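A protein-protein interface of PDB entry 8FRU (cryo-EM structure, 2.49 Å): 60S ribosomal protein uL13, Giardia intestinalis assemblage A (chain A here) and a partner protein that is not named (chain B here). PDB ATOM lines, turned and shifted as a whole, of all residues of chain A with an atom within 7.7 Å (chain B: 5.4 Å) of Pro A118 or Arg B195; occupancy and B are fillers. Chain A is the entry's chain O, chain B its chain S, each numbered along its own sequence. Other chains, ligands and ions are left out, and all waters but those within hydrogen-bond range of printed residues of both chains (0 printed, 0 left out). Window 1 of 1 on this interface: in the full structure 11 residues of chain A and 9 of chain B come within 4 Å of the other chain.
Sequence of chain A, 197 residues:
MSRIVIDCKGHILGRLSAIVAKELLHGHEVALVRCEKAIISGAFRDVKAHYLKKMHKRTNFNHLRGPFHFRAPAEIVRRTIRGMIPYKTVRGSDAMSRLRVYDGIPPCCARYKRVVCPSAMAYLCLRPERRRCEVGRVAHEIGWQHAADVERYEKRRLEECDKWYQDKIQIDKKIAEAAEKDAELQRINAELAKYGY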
ATOM      1  N   GLY A  10       0.844 -19.603  -6.914  1.00  0.00           N
ATOM      2  CA  GLY A  10      -0.003 -18.638  -6.252  1.00  0.00           C
ATOM      3  C   GLY A  10       0.253 -18.443  -4.779  1.00  0.00           C
ATOM      4  O   GLY A  10      -0.496 -17.705  -4.135  1.00  0.00           O
ATOM      5  N   HIS A  11       1.282 -19.070  -4.223  1.00  0.00           N
ATOM      6  CA  HIS A  11       1.596 -18.939  -2.810  1.00  0.00           C
ATOM      7  C   HIS A  11       2.573 -17.794  -2.576  1.00  0.00           C
ATOM      8  O   HIS A  11       3.413 -17.488  -3.421  1.00  0.00           O
ATOM      9  CB  HIS A  11       2.189 -20.240  -2.273  1.00  0.00           C
ATOM     10  CG  HIS A  11       1.209 -21.366  -2.199  1.00  0.00           C
ATOM     11  ND1 HIS A  11       0.497 -21.805  -3.292  1.00  0.00           N
ATOM     12  CD2 HIS A  11       0.832 -22.153  -1.166  1.00  0.00           C
ATOM     13  CE1 HIS A  11      -0.283 -22.808  -2.933  1.00  0.00           C
ATOM     14  NE2 HIS A  11      -0.096 -23.040  -1.648  1.00  0.00           N
ATOM     15  N   ARG A  15       5.334 -16.795   3.667  1.00  0.00           N
ATOM     16  CA  ARG A  15       4.388 -17.583   4.453  1.00  0.00           C
ATOM     17  C   ARG A  15       4.543 -19.075   4.180  1.00  0.00           C
ATOM     18  O   ARG A  15       4.523 -19.900   5.110  1.00  0.00           O
ATOM     19  CB  ARG A  15       2.967 -17.115   4.153  1.00  0.00           C
ATOM     20  CG  ARG A  15       2.851 -15.624   3.911  1.00  0.00           C
ATOM     21  CD  ARG A  15       1.474 -15.102   4.277  1.00  0.00           C
ATOM     22  NE  ARG A  15       1.522 -13.731   4.767  1.00  0.00           N
ATOM     23  CZ  ARG A  15       1.026 -13.334   5.931  1.00  0.00           C
ATOM     24  NH1 ARG A  15       0.416 -14.177   6.745  1.00  0.00           N
ATOM     25  NH2 ARG A  15       1.156 -12.063   6.292  1.00  0.00           N
ATOM     26  N   ALA A  18       7.593 -20.298   5.985  1.00  0.00           N
ATOM     27  CA  ALA A  18       7.374 -20.510   7.413  1.00  0.00           C
ATOM     28  C   ALA A  18       6.676 -21.843   7.679  1.00  0.00           C
ATOM     29  O   ALA A  18       7.106 -22.632   8.537  1.00  0.00           O
ATOM     30  CB  ALA A  18       6.573 -19.348   7.995  1.00  0.00           C
ATOM     31  N   ILE A  19       5.609 -22.124   6.926  1.00  0.00           N
ATOM     32  CA  ILE A  19       4.893 -23.387   7.113  1.00  0.00           C
ATOM     33  C   ILE A  19       5.815 -24.574   6.846  1.00  0.00           C
ATOM     34  O   ILE A  19       5.836 -25.556   7.601  1.00  0.00           O
ATOM     35  CB  ILE A  19       3.648 -23.442   6.214  1.00  0.00           C
ATOM     36  CG1 ILE A  19       2.558 -22.516   6.740  1.00  0.00           C
ATOM     37  CG2 ILE A  19       3.140 -24.858   6.117  1.00  0.00           C
ATOM     38  CD1 ILE A  19       1.393 -22.380   5.807  1.00  0.00           C
ATOM     39  N   VAL A  20       6.581 -24.508   5.757  1.00  0.00           N
ATOM     40  CA  VAL A  20       7.404 -25.646   5.371  1.00  0.00           C
ATOM     41  C   VAL A  20       8.519 -25.872   6.380  1.00  0.00           C
ATOM     42  O   VAL A  20       8.884 -27.013   6.667  1.00  0.00           O
ATOM     43  CB  VAL A  20       7.960 -25.457   3.949  1.00  0.00           C
ATOM     44  CG1 VAL A  20       9.008 -26.500   3.661  1.00  0.00           C
ATOM     45  CG2 VAL A  20       6.851 -25.547   2.941  1.00  0.00           C
ATOM     46  N   LYS A  22       8.401 -25.221   9.612  1.00  0.00           N
ATOM     47  CA  LYS A  22       7.813 -25.888  10.767  1.00  0.00           C
ATOM     48  C   LYS A  22       7.574 -27.367  10.482  1.00  0.00           C
ATOM     49  O   LYS A  22       7.845 -28.220  11.333  1.00  0.00           O
ATOM     50  CB  LYS A  22       6.519 -25.195  11.178  1.00  0.00           C
ATOM     51  CG  LYS A  22       6.164 -25.363  12.644  1.00  0.00           C
ATOM     52  CD  LYS A  22       7.380 -25.235  13.544  1.00  0.00           C
ATOM     53  CE  LYS A  22       6.975 -24.812  14.937  1.00  0.00           C
ATOM     54  NZ  LYS A  22       8.094 -24.836  15.903  1.00  0.00           N
ATOM     55  N   GLU A  23       7.074 -27.693   9.288  1.00  0.00           N
ATOM     56  CA  GLU A  23       6.860 -29.098   8.944  1.00  0.00           C
ATOM     57  C   GLU A  23       8.170 -29.878   8.919  1.00  0.00           C
ATOM     58  O   GLU A  23       8.231 -31.019   9.388  1.00  0.00           O
ATOM     59  CB  GLU A  23       6.161 -29.213   7.591  1.00  0.00           C
ATOM     60  CG  GLU A  23       4.694 -28.867   7.609  1.00  0.00           C
ATOM     61  CD  GLU A  23       3.992 -29.364   8.849  1.00  0.00           C
ATOM     62  OE1 GLU A  23       3.814 -30.592   8.977  1.00  0.00           O
ATOM     63  OE2 GLU A  23       3.608 -28.530   9.691  1.00  0.00           O
ATOM     64  N   VAL A 115      -1.150 -30.977  -2.640  1.00  0.00           N
ATOM     65  CA  VAL A 115      -2.002 -30.218  -1.743  1.00  0.00           C
ATOM     66  C   VAL A 115      -1.627 -28.746  -1.857  1.00  0.00           C
ATOM     67  O   VAL A 115      -0.682 -28.380  -2.550  1.00  0.00           O
ATOM     68  CB  VAL A 115      -1.893 -30.701  -0.281  1.00  0.00           C
ATOM     69  CG1 VAL A 115      -2.275 -32.158  -0.168  1.00  0.00           C
ATOM     70  CG2 VAL A 115      -0.498 -30.475   0.249  1.00  0.00           C
ATOM     71  N   VAL A 116      -2.389 -27.899  -1.165  1.00  0.00           N
ATOM     72  CA  VAL A 116      -2.122 -26.470  -1.092  1.00  0.00           C
ATOM     73  C   VAL A 116      -2.258 -26.024   0.358  1.00  0.00           C
ATOM     74  O   VAL A 116      -2.747 -26.756   1.216  1.00  0.00           O
ATOM     75  CB  VAL A 116      -3.060 -25.645  -1.994  1.00  0.00           C
ATOM     76  CG1 VAL A 116      -2.841 -26.001  -3.447  1.00  0.00           C
ATOM     77  CG2 VAL A 116      -4.502 -25.856  -1.596  1.00  0.00           C
ATOM     78  N   CYS A 117      -1.796 -24.806   0.622  1.00  0.00           N
ATOM     79  CA  CYS A 117      -1.998 -24.140   1.910  1.00  0.00           C
ATOM     80  C   CYS A 117      -2.736 -22.832   1.666  1.00  0.00           C
ATOM     81  O   CYS A 117      -2.105 -21.811   1.343  1.00  0.00           O
ATOM     82  CB  CYS A 117      -0.674 -23.884   2.624  1.00  0.00           C
ATOM     83  SG  CYS A 117       0.373 -25.331   2.847  1.00  0.00           S
ATOM     84  N   PRO A 118      -4.060 -22.806   1.805  1.00  0.00           N
ATOM     85  CA  PRO A 118      -4.798 -21.570   1.508  1.00  0.00           C
ATOM     86  C   PRO A 118      -4.394 -20.384   2.367  1.00  0.00           C
ATOM     87  O   PRO A 118      -4.519 -19.241   1.919  1.00  0.00           O
ATOM     88  CB  PRO A 118      -6.257 -21.977   1.746  1.00  0.00           C
ATOM     89  CG  PRO A 118      -6.262 -23.450   1.597  1.00  0.00           C
ATOM     90  CD  PRO A 118      -4.963 -23.913   2.150  1.00  0.00           C
ATOM     91  N   SER A 119      -3.900 -20.611   3.583  1.00  0.00           N
ATOM     92  CA  SER A 119      -3.523 -19.502   4.451  1.00  0.00           C
ATOM     93  C   SER A 119      -2.320 -18.725   3.937  1.00  0.00           C
ATOM     94  O   SER A 119      -2.024 -17.657   4.480  1.00  0.00           O
ATOM     95  CB  SER A 119      -3.238 -20.012   5.862  1.00  0.00           C
ATOM     96  OG  SER A 119      -2.592 -21.268   5.825  1.00  0.00           O
ATOM     97  N   ALA A 120      -1.620 -19.232   2.923  1.00  0.00           N
ATOM     98  CA  ALA A 120      -0.447 -18.576   2.360  1.00  0.00           C
ATOM     99  C   ALA A 120      -0.610 -18.262   0.879  1.00  0.00           C
ATOM    100  O   ALA A 120       0.385 -18.109   0.173  1.00  0.00           O
ATOM    101  CB  ALA A 120       0.797 -19.437   2.576  1.00  0.00           C
ATOM    102  N   MET A 121      -1.841 -18.162   0.391  1.00  0.00           N
ATOM    103  CA  MET A 121      -2.112 -17.940  -1.021  1.00  0.00           C
ATOM    104  C   MET A 121      -2.462 -16.480  -1.270  1.00  0.00           C
ATOM    105  O   MET A 121      -3.117 -15.840  -0.447  1.00  0.00           O
ATOM    106  CB  MET A 121      -3.244 -18.843  -1.497  1.00  0.00           C
ATOM    107  CG  MET A 121      -2.799 -20.247  -1.806  1.00  0.00           C
ATOM    108  SD  MET A 121      -4.150 -21.314  -2.287  1.00  0.00           S
ATOM    109  CE  MET A 121      -3.758 -21.534  -4.012  1.00  0.00           C
ATOM    110  N   ALA A 122      -2.032 -15.966  -2.422  1.00  0.00           N
ATOM    111  CA  ALA A 122      -2.069 -14.528  -2.664  1.00  0.00           C
ATOM    112  C   ALA A 122      -3.486 -13.998  -2.835  1.00  0.00           C
ATOM    113  O   ALA A 122      -3.758 -12.851  -2.472  1.00  0.00           O
ATOM    114  CB  ALA A 122      -1.224 -14.184  -3.888  1.00  0.00           C
ATOM    115  N   TYR A 123      -4.397 -14.794  -3.390  1.00  0.00           N
ATOM    116  CA  TYR A 123      -5.757 -14.309  -3.596  1.00  0.00           C
ATOM    117  C   TYR A 123      -6.545 -14.210  -2.298  1.00  0.00           C
ATOM    118  O   TYR A 123      -7.662 -13.688  -2.312  1.00  0.00           O
ATOM    119  CB  TYR A 123      -6.487 -15.194  -4.612  1.00  0.00           C
ATOM    120  CG  TYR A 123      -7.051 -16.472  -4.053  1.00  0.00           C
ATOM    121  CD1 TYR A 123      -6.229 -17.547  -3.765  1.00  0.00           C
ATOM    122  CD2 TYR A 123      -8.408 -16.606  -3.816  1.00  0.00           C
ATOM    123  CE1 TYR A 123      -6.740 -18.712  -3.255  1.00  0.00           C
ATOM    124  CE2 TYR A 123      -8.925 -17.768  -3.307  1.00  0.00           C
ATOM    125  CZ  TYR A 123      -8.086 -18.819  -3.027  1.00  0.00           C
ATOM    126  OH  TYR A 123      -8.594 -19.982  -2.516  1.00  0.00           O
ATOM    127  N   LEU A 124      -5.995 -14.689  -1.186  1.00  0.00           N
ATOM    128  CA  LEU A 124      -6.583 -14.492   0.128  1.00  0.00           C
ATOM    129  C   LEU A 124      -5.749 -13.606   1.042  1.00  0.00           C
ATOM    130  O   LEU A 124      -6.247 -13.199   2.095  1.00  0.00           O
ATOM    131  CB  LEU A 124      -6.804 -15.837   0.829  1.00  0.00           C
ATOM    132  CG  LEU A 124      -7.799 -16.823   0.229  1.00  0.00           C
ATOM    133  CD1 LEU A 124      -7.728 -18.135   0.979  1.00  0.00           C
ATOM    134  CD2 LEU A 124      -9.202 -16.264   0.261  1.00  0.00           C
ATOM    135  N   CYS A 125      -4.503 -13.296   0.680  1.00  0.00           N
ATOM    136  CA  CYS A 125      -3.606 -12.571   1.565  1.00  0.00           C
ATOM    137  C   CYS A 125      -3.361 -11.124   1.165  1.00  0.00           C
ATOM    138  O   CYS A 125      -2.917 -10.341   2.007  1.00  0.00           O
ATOM    139  CB  CYS A 125      -2.250 -13.287   1.656  1.00  0.00           C
ATOM    140  SG  CYS A 125      -2.215 -14.718   2.755  1.00  0.00           S
ATOM    141  N   ALA B 191      -8.941 -21.952   7.077  1.00  0.00           N
ATOM    142  CA  ALA B 191      -7.657 -22.520   6.699  1.00  0.00           C
ATOM    143  C   ALA B 191      -6.692 -22.629   7.868  1.00  0.00           C
ATOM    144  O   ALA B 191      -5.679 -23.323   7.751  1.00  0.00           O
ATOM    145  CB  ALA B 191      -7.022 -21.691   5.585  1.00  0.00           C
ATOM    146  N   ARG B 192      -6.969 -21.957   8.984  1.00  0.00           N
ATOM    147  CA  ARG B 192      -6.067 -22.041  10.124  1.00  0.00           C
ATOM    148  C   ARG B 192      -6.079 -23.429  10.745  1.00  0.00           C
ATOM    149  O   ARG B 192      -5.044 -23.900  11.226  1.00  0.00           O
ATOM    150  CB  ARG B 192      -6.430 -20.985  11.163  1.00  0.00           C
ATOM    151  CG  ARG B 192      -5.655 -21.120  12.454  1.00  0.00           C
ATOM    152  CD  ARG B 192      -5.100 -19.792  12.942  1.00  0.00           C
ATOM    153  NE  ARG B 192      -5.950 -18.661  12.598  1.00  0.00           N
ATOM    154  CZ  ARG B 192      -7.088 -18.364  13.208  1.00  0.00           C
ATOM    155  NH1 ARG B 192      -7.583 -19.135  14.159  1.00  0.00           N
ATOM    156  NH2 ARG B 192      -7.751 -17.271  12.848  1.00  0.00           N
ATOM    157  N   THR B 193      -7.228 -24.097  10.745  1.00  0.00           N
ATOM    158  CA  THR B 193      -7.321 -25.444  11.290  1.00  0.00           C
ATOM    159  C   THR B 193      -7.025 -26.512  10.246  1.00  0.00           C
ATOM    160  O   THR B 193      -6.336 -27.491  10.544  1.00  0.00           O
ATOM    161  CB  THR B 193      -8.708 -25.672  11.893  1.00  0.00           C
ATOM    162  OG1 THR B 193      -8.913 -27.072  12.113  1.00  0.00           O
ATOM    163  CG2 THR B 193      -9.787 -25.146  10.960  1.00  0.00           C
ATOM    164  N   ALA B 194      -7.525 -26.344   9.025  1.00  0.00           N
ATOM    165  CA  ALA B 194      -7.235 -27.260   7.924  1.00  0.00           C
ATOM    166  C   ALA B 194      -6.059 -26.695   7.139  1.00  0.00           C
ATOM    167  O   ALA B 194      -6.226 -25.948   6.178  1.00  0.00           O
ATOM    168  CB  ALA B 194      -8.462 -27.456   7.042  1.00  0.00           C
ATOM    169  N   ARG B 195      -4.849 -27.068   7.558  1.00  0.00           N
ATOM    170  CA  ARG B 195      -3.639 -26.489   6.984  1.00  0.00           C
ATOM    171  C   ARG B 195      -3.468 -26.876   5.519  1.00  0.00           C
ATOM    172  O   ARG B 195      -3.251 -26.015   4.661  1.00  0.00           O
ATOM    173  CB  ARG B 195      -2.425 -26.932   7.797  1.00  0.00           C
ATOM    174  CG  ARG B 195      -1.214 -26.030   7.686  1.00  0.00           C
ATOM    175  CD  ARG B 195      -0.216 -26.350   8.780  1.00  0.00           C
ATOM    176  NE  ARG B 195       0.611 -25.203   9.129  1.00  0.00           N
ATOM    177  CZ  ARG B 195       0.195 -24.177   9.856  1.00  0.00           C
ATOM    178  NH1 ARG B 195      -1.039 -24.122  10.330  1.00  0.00           N
ATOM    179  NH2 ARG B 195       1.034 -23.177  10.107  1.00  0.00           N
ATOM    180  N   PHE B 196      -3.559 -28.164   5.214  1.00  0.00           N
ATOM    181  CA  PHE B 196      -3.324 -28.677   3.873  1.00  0.00           C
ATOM    182  C   PHE B 196      -4.628 -29.203   3.299  1.00  0.00           C
ATOM    183  O   PHE B 196      -5.303 -30.022   3.928  1.00  0.00           O
ATOM    184  CB  PHE B 196      -2.259 -29.775   3.888  1.00  0.00           C
ATOM    185  CG  PHE B 196      -0.959 -29.344   4.495  1.00  0.00           C
ATOM    186  CD1 PHE B 196      -0.018 -28.674   3.740  1.00  0.00           C
ATOM    187  CD2 PHE B 196      -0.679 -29.602   5.822  1.00  0.00           C
ATOM    188  CE1 PHE B 196       1.174 -28.271   4.297  1.00  0.00           C
ATOM    189  CE2 PHE B 196       0.513 -29.200   6.383  1.00  0.00           C
ATOM    190  CZ  PHE B 196       1.441 -28.535   5.620  1.00  0.00           C
ATOM    191  N   GLN B 197      -4.977 -28.729   2.109  1.00  0.00           N
ATOM    192  CA  GLN B 197      -6.240 -29.047   1.469  1.00  0.00           C
ATOM    193  C   GLN B 197      -5.966 -29.523   0.052  1.00  0.00           C
ATOM    194  O   GLN B 197      -4.917 -29.234  -0.524  1.00  0.00           O
ATOM    195  CB  GLN B 197      -7.171 -27.834   1.467  1.00  0.00           C
ATOM    196  CG  GLN B 197      -7.811 -27.561   2.813  1.00  0.00           C
ATOM    197  CD  GLN B 197      -8.494 -26.217   2.874  1.00  0.00           C
ATOM    198  OE1 GLN B 197      -9.274 -25.869   1.996  1.00  0.00           O
ATOM    199  NE2 GLN B 197      -8.219 -25.460   3.921  1.00  0.00           N
ATOM    200  N   ARG B 199      -7.664 -28.810  -2.718  1.00  0.00           N
ATOM    201  CA  ARG B 199      -7.923 -27.839  -3.771  1.00  0.00           C
ATOM    202  C   ARG B 199      -8.059 -26.467  -3.136  1.00  0.00           C
ATOM    203  O   ARG B 199      -8.290 -26.344  -1.933  1.00  0.00           O
ATOM    204  CB  ARG B 199      -9.175 -28.191  -4.581  1.00  0.00           C
ATOM    205  CG  ARG B 199     -10.459 -27.538  -4.097  1.00  0.00           C
ATOM    206  CD  ARG B 199     -11.137 -28.392  -3.059  1.00  0.00           C
ATOM    207  NE  ARG B 199     -12.084 -27.645  -2.244  1.00  0.00           N
ATOM    208  CZ  ARG B 199     -11.802 -27.128  -1.056  1.00  0.00           C
ATOM    209  NH1 ARG B 199     -10.588 -27.205  -0.541  1.00  0.00           N
ATOM    210  NH2 ARG B 199     -12.764 -26.528  -0.364  1.00  0.00           N
ATOM    211  N   PRO B 201     -10.044 -23.435  -2.147  1.00  0.00           N
ATOM    212  CA  PRO B 201     -11.469 -23.132  -1.988  1.00  0.00           C
ATOM    213  C   PRO B 201     -11.869 -21.848  -2.697  1.00  0.00           C
ATOM    214  O   PRO B 201     -11.098 -20.894  -2.791  1.00  0.00           O
ATOM    215  CB  PRO B 201     -11.633 -22.999  -0.472  1.00  0.00           C
ATOM    216  CG  PRO B 201     -10.276 -22.670   0.025  1.00  0.00           C
ATOM    217  CD  PRO B 201      -9.314 -23.361  -0.874  1.00  0.00           C
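O of Gln B197 lies within hydrogen-bond range of N of Val A116.
O of Pro B201 lies within hydrogen-bond range of OH of Tyr A123, at 2.7 Å.
A ring nitrogen (NE2) of His A11 lies within hydrogen-bond range of the backbone NH of Cys A117 (3.3 Å).
The backbone carbonyl oxygen (O) of Ser A119 sits at hydrogen-bond distance from the side-chain sulfur (SG) of Cys A125 (3.4 Å).
NE2 of Gln B197 lies within hydrogen-bond range of O of Ala B194 (3.1 Å).
The guanidinium group (NH1) of Arg B199 is in hydrogen-bond range of the side-chain amide oxygen (OE1) of Gln B197 (3.2 Å).
Among the printed residues, merely in contact across the chains: Val A115 with Gln B197 (3.3 Å), Val A116 with Phe B196 (3.3 Å), Cys A117 with Phe B196 (3.4 Å), Cys A117 with Arg B195 (3.6 Å), Val A116 with Arg B195 (3.6 Å), Pro A118 with Gln B197 (3.6 Å), Pro A118 with Arg B195 (3.7 Å), Ile A19 with Arg B195 (3.8 Å), Glu A23 with Phe B196 (3.8 Å), Val A116 with Arg B199 (3.8 Å), Ser A119 with Ala B191 (3.9 Å), Pro A118 with Ala B191 (3.9 Å), Pro A118 with Pro B201 (3.9 Å) and Val A115 with Phe B196 (3.96 Å).
Of chain B, only Ala B191 (3.9 Å), Arg B195 (3.7 Å), Gln B197 (3.6 Å) and Pro B201 (3.9 Å) come within 4 Å of Pro A118.
Arg B195 touches just these residues of chain A: Ile A19 (3.8 Å), Val A116 (3.6 Å), Cys A117 (3.6 Å) and Pro A118 (3.7 Å).
Of the printed residues of chain A, Pro B201 touches Pro A118 and Tyr A123.
Printed residues of chain B within 4 Å of Cys A117: Arg B195 (3.6 Å) and Phe B196 (3.4 Å).
Of the printed residues of chain A, Ala B191 touches Pro A118 and Ser A119.
Ala A120 touches none of the printed residues of chain B.
Hydrophobic or aromatic side chains of chain A within 4 Å of the printed part of chain B: Ile A19, Val A115, Val A116, Pro A118 and Tyr A123.
Of the 9 printed residues of chain B, 6 touch a printed residue of chain A.
Hydrophobic or aromatic side chains of chain B within 4 Å of the printed part of chain A: Ala B191, Phe B196 and Pro B201.
Among the printed residues, no Asp or Glu carboxylate lies within 4 Å of a Lys or Arg side-chain nitrogen of the other chain.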
